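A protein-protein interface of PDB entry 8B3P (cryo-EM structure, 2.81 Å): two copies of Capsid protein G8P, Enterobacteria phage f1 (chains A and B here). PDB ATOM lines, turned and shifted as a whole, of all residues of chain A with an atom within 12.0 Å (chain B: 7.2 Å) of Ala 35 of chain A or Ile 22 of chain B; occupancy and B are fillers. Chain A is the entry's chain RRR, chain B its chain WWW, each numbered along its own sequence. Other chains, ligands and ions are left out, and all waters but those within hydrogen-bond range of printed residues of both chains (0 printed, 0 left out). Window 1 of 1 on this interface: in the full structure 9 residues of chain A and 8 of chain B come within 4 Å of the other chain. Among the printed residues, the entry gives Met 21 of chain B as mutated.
Among the printed residues, merely in contact across the chains: Met 28 of chain A with Gln 15 of chain B, Ala 35 of chain A with Ile 22 of chain B, Ala 27 of chain A with Gln 15 of chain B, Ile 39 of chain A with Trp 26 of chain B, Gly 38 of chain A with Trp 26 of chain B and Val 31 of chain A with Ile 22 of chain B.
Of the printed residues of chain B, Ala 35 of chain A touches Ile 22 (3.7 Å).
Of the printed residues of chain A, Ile 22 of chain B touches Val 31 (3.98 Å) and Ala 35 (3.7 Å).
No residue of chain B comes within 4 Å of Gly 34 of chain A.
Met 21 of chain B touches none of the printed residues of chain A.
Gly 23 of chain B touches none of the printed residues of chain A.
No residue of chain A comes within 4 Å of Tyr 24 of chain B.
Ala 25 of chain B touches none of the printed residues of chain A.
Of chain A, only Gly 38 (3.98 Å) and Ile 39 (3.8 Å) come within 4 Å of Trp 26 of chain B.
Of the printed residues of chain B, Val 31 of chain A touches Ile 22.
Of the printed residues of chain B, Met 28 of chain A touches Gln 15 (3.6 Å).
Of the printed residues of chain A, Gln 15 of chain B touches Ala 27 (3.7 Å) and Met 28 (3.6 Å).
Ile 37 of chain A touches none of the printed residues of chain B.
Ser 17 of chain B touches none of the printed residues of chain A.
The nearest printed residue of chain A that does not touch Ile 22 of chain B is Ile 32 of chain A (4.6 Å).
The nearest printed residue of chain A that does not touch Gln 15 of chain B is Val 31 of chain A (4.9 Å).
Positions printed for both chains: 26 and 27.
Of the 6 pairs that touch across the chains among the printed residues, none has its exchanged pair printed and touching as well.
Of the 12 printed residues of chain B, 3 touch a printed residue of chain A.
Printed residues of chain B that touch a printed residue of chain A: Gln 15, Ile 22 and Trp 26.
Hydrophobic or aromatic side chains of chain B that line the printed part of chain A: Ile 22 and Trp 26.
Of the 19 printed residues of chain A, 6 touch a printed residue of chain B.
Printed residues of chain A that touch a printed residue of chain B: Ala 27, Met 28, Val 31, Ala 35, Gly 38 and Ile 39.
Hydrophobic or aromatic side chains of chain A within 4 Å of the printed part of chain B: Ala 27, Met 28, Val 31, Ala 35 and Ile 39.
Among the printed residues, 6 pairs touch across the chains.
OG1 of Thr 19 of chain B lies within hydrogen-bond range of O of Gln 15 of chain B, 2.8 Å away.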
ATOM      1  N   TRP A  26      27.651   7.098 -23.656  1.00  0.00           N
ATOM      2  CA  TRP A  26      27.236   8.124 -24.606  1.00  0.00           C
ATOM      3  C   TRP A  26      26.454   9.232 -23.907  1.00  0.00           C
ATOM      4  O   TRP A  26      26.567  10.397 -24.296  1.00  0.00           O
ATOM      5  CB  TRP A  26      26.493   7.550 -25.829  1.00  0.00           C
ATOM      6  CG  TRP A  26      27.410   7.276 -26.985  1.00  0.00           C
ATOM      7  CD1 TRP A  26      27.877   6.060 -27.399  1.00  0.00           C
ATOM      8  CD2 TRP A  26      28.028   8.250 -27.846  1.00  0.00           C
ATOM      9  NE1 TRP A  26      28.731   6.206 -28.459  1.00  0.00           N
ATOM     10  CE2 TRP A  26      28.846   7.538 -28.755  1.00  0.00           C
ATOM     11  CE3 TRP A  26      27.970   9.647 -27.948  1.00  0.00           C
ATOM     12  CZ2 TRP A  26      29.590   8.178 -29.747  1.00  0.00           C
ATOM     13  CZ3 TRP A  26      28.708  10.280 -28.926  1.00  0.00           C
ATOM     14  CH2 TRP A  26      29.509   9.553 -29.811  1.00  0.00           C
ATOM     15  N   ALA A  27      25.697   8.858 -22.865  1.00  0.00           N
ATOM     16  CA  ALA A  27      24.865   9.793 -22.120  1.00  0.00           C
ATOM     17  C   ALA A  27      25.732  10.763 -21.319  1.00  0.00           C
ATOM     18  O   ALA A  27      25.460  11.962 -21.313  1.00  0.00           O
ATOM     19  CB  ALA A  27      23.898   9.049 -21.236  1.00  0.00           C
ATOM     20  N   MET A  28      26.768  10.231 -20.657  1.00  0.00           N
ATOM     21  CA  MET A  28      27.668  11.025 -19.843  1.00  0.00           C
ATOM     22  C   MET A  28      28.436  12.014 -20.716  1.00  0.00           C
ATOM     23  O   MET A  28      28.508  13.189 -20.380  1.00  0.00           O
ATOM     24  CB  MET A  28      28.653  10.150 -19.066  1.00  0.00           C
ATOM     25  CG  MET A  28      29.271  10.889 -17.897  1.00  0.00           C
ATOM     26  SD  MET A  28      29.960   9.818 -16.639  1.00  0.00           S
ATOM     27  CE  MET A  28      28.450   9.122 -15.968  1.00  0.00           C
ATOM     28  N   VAL A  29      28.995  11.541 -21.838  1.00  0.00           N
ATOM     29  CA  VAL A  29      29.858  12.381 -22.653  1.00  0.00           C
ATOM     30  C   VAL A  29      29.096  13.622 -23.122  1.00  0.00           C
ATOM     31  O   VAL A  29      29.642  14.723 -23.091  1.00  0.00           O
ATOM     32  CB  VAL A  29      30.531  11.610 -23.806  1.00  0.00           C
ATOM     33  CG1 VAL A  29      29.587  11.359 -24.966  1.00  0.00           C
ATOM     34  CG2 VAL A  29      31.768  12.347 -24.296  1.00  0.00           C
ATOM     35  N   VAL A  30      27.820  13.437 -23.488  1.00  0.00           N
ATOM     36  CA  VAL A  30      27.009  14.519 -24.019  1.00  0.00           C
ATOM     37  C   VAL A  30      26.916  15.654 -22.995  1.00  0.00           C
ATOM     38  O   VAL A  30      27.063  16.818 -23.366  1.00  0.00           O
ATOM     39  CB  VAL A  30      25.637  14.019 -24.521  1.00  0.00           C
ATOM     40  CG1 VAL A  30      24.596  15.126 -24.651  1.00  0.00           C
ATOM     41  CG2 VAL A  30      25.767  13.272 -25.840  1.00  0.00           C
ATOM     42  N   VAL A  31      26.730  15.301 -21.710  1.00  0.00           N
ATOM     43  CA  VAL A  31      26.479  16.268 -20.646  1.00  0.00           C
ATOM     44  C   VAL A  31      27.757  17.061 -20.362  1.00  0.00           C
ATOM     45  O   VAL A  31      27.703  18.290 -20.298  1.00  0.00           O
ATOM     46  CB  VAL A  31      25.842  15.627 -19.387  1.00  0.00           C
ATOM     47  CG1 VAL A  31      25.889  16.500 -18.138  1.00  0.00           C
ATOM     48  CG2 VAL A  31      24.416  15.150 -19.646  1.00  0.00           C
ATOM     49  N   ILE A  32      28.889  16.359 -20.224  1.00  0.00           N
ATOM     50  CA  ILE A  32      30.167  16.994 -19.943  1.00  0.00           C
ATOM     51  C   ILE A  32      30.530  17.948 -21.085  1.00  0.00           C
ATOM     52  O   ILE A  32      30.878  19.101 -20.828  1.00  0.00           O
ATOM     53  CB  ILE A  32      31.281  15.957 -19.680  1.00  0.00           C
ATOM     54  CG1 ILE A  32      31.017  15.076 -18.452  1.00  0.00           C
ATOM     55  CG2 ILE A  32      32.652  16.624 -19.631  1.00  0.00           C
ATOM     56  CD1 ILE A  32      31.350  15.699 -17.109  1.00  0.00           C
ATOM     57  N   VAL A  33      30.429  17.473 -22.335  1.00  0.00           N
ATOM     58  CA  VAL A  33      30.867  18.267 -23.478  1.00  0.00           C
ATOM     59  C   VAL A  33      29.968  19.495 -23.641  1.00  0.00           C
ATOM     60  O   VAL A  33      30.457  20.571 -23.967  1.00  0.00           O
ATOM     61  CB  VAL A  33      30.988  17.440 -24.778  1.00  0.00           C
ATOM     62  CG1 VAL A  33      31.054  18.304 -26.032  1.00  0.00           C
ATOM     63  CG2 VAL A  33      32.182  16.495 -24.734  1.00  0.00           C
ATOM     64  N   GLY A  34      28.661  19.323 -23.409  1.00  0.00           N
ATOM     65  CA  GLY A  34      27.710  20.424 -23.412  1.00  0.00           C
ATOM     66  C   GLY A  34      28.187  21.603 -22.566  1.00  0.00           C
ATOM     67  O   GLY A  34      28.178  22.745 -23.035  1.00  0.00           O
ATOM     68  N   ALA A  35      28.621  21.292 -21.335  1.00  0.00           N
ATOM     69  CA  ALA A  35      29.069  22.267 -20.348  1.00  0.00           C
ATOM     70  C   ALA A  35      30.340  22.968 -20.814  1.00  0.00           C
ATOM     71  O   ALA A  35      30.397  24.196 -20.825  1.00  0.00           O
ATOM     72  CB  ALA A  35      29.288  21.585 -19.024  1.00  0.00           C
ATOM     73  N   THR A  36      31.343  22.167 -21.190  1.00  0.00           N
ATOM     74  CA  THR A  36      32.638  22.647 -21.645  1.00  0.00           C
ATOM     75  C   THR A  36      32.473  23.679 -22.760  1.00  0.00           C
ATOM     76  O   THR A  36      32.999  24.783 -22.635  1.00  0.00           O
ATOM     77  CB  THR A  36      33.543  21.478 -22.050  1.00  0.00           C
ATOM     78  OG1 THR A  36      33.651  20.625 -20.911  1.00  0.00           O
ATOM     79  CG2 THR A  36      34.922  21.910 -22.494  1.00  0.00           C
ATOM     80  N   ILE A  37      31.725  23.321 -23.818  1.00  0.00           N
ATOM     81  CA  ILE A  37      31.585  24.151 -25.008  1.00  0.00           C
ATOM     82  C   ILE A  37      30.782  25.401 -24.652  1.00  0.00           C
ATOM     83  O   ILE A  37      31.100  26.497 -25.122  1.00  0.00           O
ATOM     84  CB  ILE A  37      30.982  23.361 -26.200  1.00  0.00           C
ATOM     85  CG1 ILE A  37      31.901  22.241 -26.704  1.00  0.00           C
ATOM     86  CG2 ILE A  37      30.554  24.268 -27.349  1.00  0.00           C
ATOM     87  CD1 ILE A  37      33.354  22.636 -26.868  1.00  0.00           C
ATOM     88  N   GLY A  38      29.748  25.210 -23.820  1.00  0.00           N
ATOM     89  CA  GLY A  38      28.910  26.297 -23.342  1.00  0.00           C
ATOM     90  C   GLY A  38      29.736  27.417 -22.713  1.00  0.00           C
ATOM     91  O   GLY A  38      29.577  28.587 -23.075  1.00  0.00           O
ATOM     92  N   ILE A  39      30.633  27.035 -21.792  1.00  0.00           N
ATOM     93  CA  ILE A  39      31.444  27.990 -21.054  1.00  0.00           C
ATOM     94  C   ILE A  39      32.395  28.704 -22.013  1.00  0.00           C
ATOM     95  O   ILE A  39      32.526  29.926 -21.945  1.00  0.00           O
ATOM     96  CB  ILE A  39      32.133  27.329 -19.840  1.00  0.00           C
ATOM     97  CG1 ILE A  39      31.104  27.015 -18.745  1.00  0.00           C
ATOM     98  CG2 ILE A  39      33.270  28.187 -19.301  1.00  0.00           C
ATOM     99  CD1 ILE A  39      31.569  26.032 -17.686  1.00  0.00           C
ATOM    100  N   LYS A  40      32.993  27.937 -22.932  1.00  0.00           N
ATOM    101  CA  LYS A  40      33.929  28.460 -23.915  1.00  0.00           C
ATOM    102  C   LYS A  40      33.274  29.570 -24.738  1.00  0.00           C
ATOM    103  O   LYS A  40      33.855  30.646 -24.877  1.00  0.00           O
ATOM    104  CB  LYS A  40      34.472  27.328 -24.792  1.00  0.00           C
ATOM    105  CG  LYS A  40      35.494  27.728 -25.843  1.00  0.00           C
ATOM    106  CD  LYS A  40      35.690  26.640 -26.874  1.00  0.00           C
ATOM    107  CE  LYS A  40      36.933  26.824 -27.714  1.00  0.00           C
ATOM    108  NZ  LYS A  40      37.217  25.621 -28.534  1.00  0.00           N
ATOM    109  N   LEU A  41      32.061  29.317 -25.253  1.00  0.00           N
ATOM    110  CA  LEU A  41      31.388  30.276 -26.118  1.00  0.00           C
ATOM    111  C   LEU A  41      30.972  31.528 -25.345  1.00  0.00           C
ATOM    112  O   LEU A  41      31.051  32.633 -25.887  1.00  0.00           O
ATOM    113  CB  LEU A  41      30.192  29.613 -26.811  1.00  0.00           C
ATOM    114  CG  LEU A  41      30.527  28.609 -27.919  1.00  0.00           C
ATOM    115  CD1 LEU A  41      29.258  28.072 -28.561  1.00  0.00           C
ATOM    116  CD2 LEU A  41      31.425  29.223 -28.986  1.00  0.00           C
ATOM    117  N   PHE A  42      30.541  31.337 -24.087  1.00  0.00           N
ATOM    118  CA  PHE A  42      30.163  32.436 -23.210  1.00  0.00           C
ATOM    119  C   PHE A  42      31.320  33.425 -23.095  1.00  0.00           C
ATOM    120  O   PHE A  42      31.158  34.604 -23.394  1.00  0.00           O
ATOM    121  CB  PHE A  42      29.714  31.927 -21.837  1.00  0.00           C
ATOM    122  CG  PHE A  42      29.330  33.020 -20.870  1.00  0.00           C
ATOM    123  CD1 PHE A  42      28.177  33.772 -21.064  1.00  0.00           C
ATOM    124  CD2 PHE A  42      30.125  33.309 -19.764  1.00  0.00           C
ATOM    125  CE1 PHE A  42      27.827  34.779 -20.174  1.00  0.00           C
ATOM    126  CE2 PHE A  42      29.782  34.325 -18.881  1.00  0.00           C
ATOM    127  CZ  PHE A  42      28.630  35.056 -19.086  1.00  0.00           C
ATOM    128  N   LYS A  43      32.501  32.907 -22.730  1.00  0.00           N
ATOM    129  CA  LYS A  43      33.697  33.715 -22.553  1.00  0.00           C
ATOM    130  C   LYS A  43      34.030  34.481 -23.832  1.00  0.00           C
ATOM    131  O   LYS A  43      34.366  35.661 -23.760  1.00  0.00           O
ATOM    132  CB  LYS A  43      34.861  32.859 -22.050  1.00  0.00           C
ATOM    133  CG  LYS A  43      34.789  32.519 -20.566  1.00  0.00           C
ATOM    134  CD  LYS A  43      35.650  31.359 -20.117  1.00  0.00           C
ATOM    135  CE  LYS A  43      37.072  31.736 -19.764  1.00  0.00           C
ATOM    136  NZ  LYS A  43      37.942  30.536 -19.716  1.00  0.00           N
ATOM    137  N   LYS A  44      33.896  33.813 -24.986  1.00  0.00           N
ATOM    138  CA  LYS A  44      34.288  34.363 -26.278  1.00  0.00           C
ATOM    139  C   LYS A  44      33.382  35.530 -26.673  1.00  0.00           C
ATOM    140  O   LYS A  44      33.873  36.616 -26.989  1.00  0.00           O
ATOM    141  CB  LYS A  44      34.308  33.261 -27.343  1.00  0.00           C
ATOM    142  CG  LYS A  44      34.476  33.735 -28.783  1.00  0.00           C
ATOM    143  CD  LYS A  44      34.692  32.628 -29.793  1.00  0.00           C
ATOM    144  CE  LYS A  44      36.100  32.634 -30.353  1.00  0.00           C
ATOM    145  NZ  LYS A  44      36.216  31.778 -31.557  1.00  0.00           N
ATOM    146  N   GLN B  15      26.880  10.411 -13.009  1.00  0.00           N
ATOM    147  CA  GLN B  15      26.206  11.446 -13.776  1.00  0.00           C
ATOM    148  C   GLN B  15      25.618  12.511 -12.855  1.00  0.00           C
ATOM    149  O   GLN B  15      25.678  13.690 -13.184  1.00  0.00           O
ATOM    150  CB  GLN B  15      25.131  10.863 -14.685  1.00  0.00           C
ATOM    151  CG  GLN B  15      24.976  11.664 -15.968  1.00  0.00           C
ATOM    152  CD  GLN B  15      23.810  11.224 -16.820  1.00  0.00           C
ATOM    153  OE1 GLN B  15      23.971  10.529 -17.822  1.00  0.00           O
ATOM    154  NE2 GLN B  15      22.614  11.637 -16.429  1.00  0.00           N
ATOM    155  N   SER B  17      26.647  13.388  -9.736  1.00  0.00           N
ATOM    156  CA  SER B  17      27.738  14.166  -9.166  1.00  0.00           C
ATOM    157  C   SER B  17      28.251  15.211 -10.158  1.00  0.00           C
ATOM    158  O   SER B  17      28.526  16.341  -9.760  1.00  0.00           O
ATOM    159  CB  SER B  17      28.852  13.273  -8.670  1.00  0.00           C
ATOM    160  OG  SER B  17      29.978  14.031  -8.252  1.00  0.00           O
ATOM    161  N   ALA B  18      28.367  14.827 -11.437  1.00  0.00           N
ATOM    162  CA  ALA B  18      28.875  15.699 -12.486  1.00  0.00           C
ATOM    163  C   ALA B  18      27.913  16.858 -12.741  1.00  0.00           C
ATOM    164  O   ALA B  18      28.359  17.967 -13.012  1.00  0.00           O
ATOM    165  CB  ALA B  18      29.144  14.915 -13.747  1.00  0.00           C
ATOM    166  N   THR B  19      26.606  16.606 -12.616  1.00  0.00           N
ATOM    167  CA  THR B  19      25.591  17.622 -12.848  1.00  0.00           C
ATOM    168  C   THR B  19      25.682  18.729 -11.796  1.00  0.00           C
ATOM    169  O   THR B  19      25.498  19.902 -12.126  1.00  0.00           O
ATOM    170  CB  THR B  19      24.209  16.971 -12.964  1.00  0.00           C
ATOM    171  OG1 THR B  19      24.325  16.025 -14.026  1.00  0.00           O
ATOM    172  CG2 THR B  19      23.097  17.948 -13.272  1.00  0.00           C
ATOM    173  N   GLU B  20      25.981  18.353 -10.544  1.00  0.00           N
ATOM    174  CA  GLU B  20      26.098  19.323  -9.464  1.00  0.00           C
ATOM    175  C   GLU B  20      27.317  20.211  -9.699  1.00  0.00           C
ATOM    176  O   GLU B  20      27.245  21.420  -9.481  1.00  0.00           O
ATOM    177  CB  GLU B  20      26.248  18.657  -8.096  1.00  0.00           C
ATOM    178  CG  GLU B  20      25.084  17.772  -7.691  1.00  0.00           C
ATOM    179  CD  GLU B  20      25.482  16.591  -6.818  1.00  0.00           C
ATOM    180  OE1 GLU B  20      26.554  16.653  -6.175  1.00  0.00           O
ATOM    181  OE2 GLU B  20      24.725  15.598  -6.792  1.00  0.00           O
ATOM    182  N   MET B  21      28.428  19.591 -10.117  1.00  0.00           N
ATOM    183  CA  MET B  21      29.685  20.294 -10.305  1.00  0.00           C
ATOM    184  C   MET B  21      29.580  21.299 -11.447  1.00  0.00           C
ATOM    185  O   MET B  21      30.132  22.384 -11.332  1.00  0.00           O
ATOM    186  CB  MET B  21      30.852  19.344 -10.563  1.00  0.00           C
ATOM    187  CG  MET B  21      31.556  18.962  -9.288  1.00  0.00           C
ATOM    188  SD  MET B  21      32.922  17.818  -9.559  1.00  0.00           S
ATOM    189  CE  MET B  21      32.032  16.328 -10.015  1.00  0.00           C
ATOM    190  N   ILE B  22      28.851  20.956 -12.516  1.00  0.00           N
ATOM    191  CA  ILE B  22      28.640  21.862 -13.635  1.00  0.00           C
ATOM    192  C   ILE B  22      27.869  23.092 -13.153  1.00  0.00           C
ATOM    193  O   ILE B  22      28.106  24.198 -13.636  1.00  0.00           O
ATOM    194  CB  ILE B  22      27.973  21.116 -14.810  1.00  0.00           C
ATOM    195  CG1 ILE B  22      28.954  20.111 -15.414  1.00  0.00           C
ATOM    196  CG2 ILE B  22      27.428  22.068 -15.869  1.00  0.00           C
ATOM    197  CD1 ILE B  22      28.297  18.972 -16.151  1.00  0.00           C
ATOM    198  N   GLY B  23      26.987  22.885 -12.166  1.00  0.00           N
ATOM    199  CA  GLY B  23      26.219  23.952 -11.544  1.00  0.00           C
ATOM    200  C   GLY B  23      27.096  24.963 -10.805  1.00  0.00           C
ATOM    201  O   GLY B  23      26.867  26.169 -10.911  1.00  0.00           O
ATOM    202  N   TYR B  24      28.097  24.457 -10.065  1.00  0.00           N
ATOM    203  CA  TYR B  24      29.011  25.291  -9.298  1.00  0.00           C
ATOM    204  C   TYR B  24      29.908  26.082 -10.241  1.00  0.00           C
ATOM    205  O   TYR B  24      30.178  27.248  -9.975  1.00  0.00           O
ATOM    206  CB  TYR B  24      29.885  24.491  -8.326  1.00  0.00           C
ATOM    207  CG  TYR B  24      29.172  23.565  -7.370  1.00  0.00           C
ATOM    208  CD1 TYR B  24      28.018  23.955  -6.696  1.00  0.00           C
ATOM    209  CD2 TYR B  24      29.673  22.293  -7.119  1.00  0.00           C
ATOM    210  CE1 TYR B  24      27.356  23.091  -5.835  1.00  0.00           C
ATOM    211  CE2 TYR B  24      29.028  21.420  -6.254  1.00  0.00           C
ATOM    212  CZ  TYR B  24      27.865  21.821  -5.612  1.00  0.00           C
ATOM    213  OH  TYR B  24      27.223  20.965  -4.763  1.00  0.00           O
ATOM    214  N   ALA B  25      30.360  25.439 -11.326  1.00  0.00           N
ATOM    215  CA  ALA B  25      31.267  26.041 -12.295  1.00  0.00           C
ATOM    216  C   ALA B  25      30.622  27.246 -12.975  1.00  0.00           C
ATOM    217  O   ALA B  25      31.291  28.256 -13.184  1.00  0.00           O
ATOM    218  CB  ALA B  25      31.712  25.013 -13.306  1.00  0.00           C
ATOM    219  N   TRP B  26      29.324  27.134 -13.295  1.00  0.00           N
ATOM    220  CA  TRP B  26      28.601  28.212 -13.952  1.00  0.00           C
ATOM    221  C   TRP B  26      28.519  29.433 -13.041  1.00  0.00           C
ATOM    222  O   TRP B  26      28.555  30.553 -13.537  1.00  0.00           O
ATOM    223  CB  TRP B  26      27.220  27.775 -14.466  1.00  0.00           C
ATOM    224  CG  TRP B  26      27.232  27.344 -15.901  1.00  0.00           C
ATOM    225  CD1 TRP B  26      27.166  26.066 -16.375  1.00  0.00           C
ATOM    226  CD2 TRP B  26      27.349  28.192 -17.058  1.00  0.00           C
ATOM    227  NE1 TRP B  26      27.223  26.057 -17.744  1.00  0.00           N
ATOM    228  CE2 TRP B  26      27.343  27.344 -18.191  1.00  0.00           C
ATOM    229  CE3 TRP B  26      27.458  29.576 -17.251  1.00  0.00           C
ATOM    230  CZ2 TRP B  26      27.441  27.840 -19.492  1.00  0.00           C
ATOM    231  CZ3 TRP B  26      27.552  30.066 -18.536  1.00  0.00           C
ATOM    232  CH2 TRP B  26      27.545  29.207 -19.640  1.00  0.00           C
ATOM    233  N   ALA B  27      28.439  29.201 -11.722  1.00  0.00           N
ATOM    234  CA  ALA B  27      28.315  30.265 -10.736  1.00  0.00           C
ATOM    235  C   ALA B  27      29.606  31.076 -10.643  1.00  0.00           C
ATOM    236  O   ALA B  27      29.560  32.302 -10.607  1.00  0.00           O
ATOM    237  CB  ALA B  27      27.926  29.693  -9.400  1.00  0.00           C
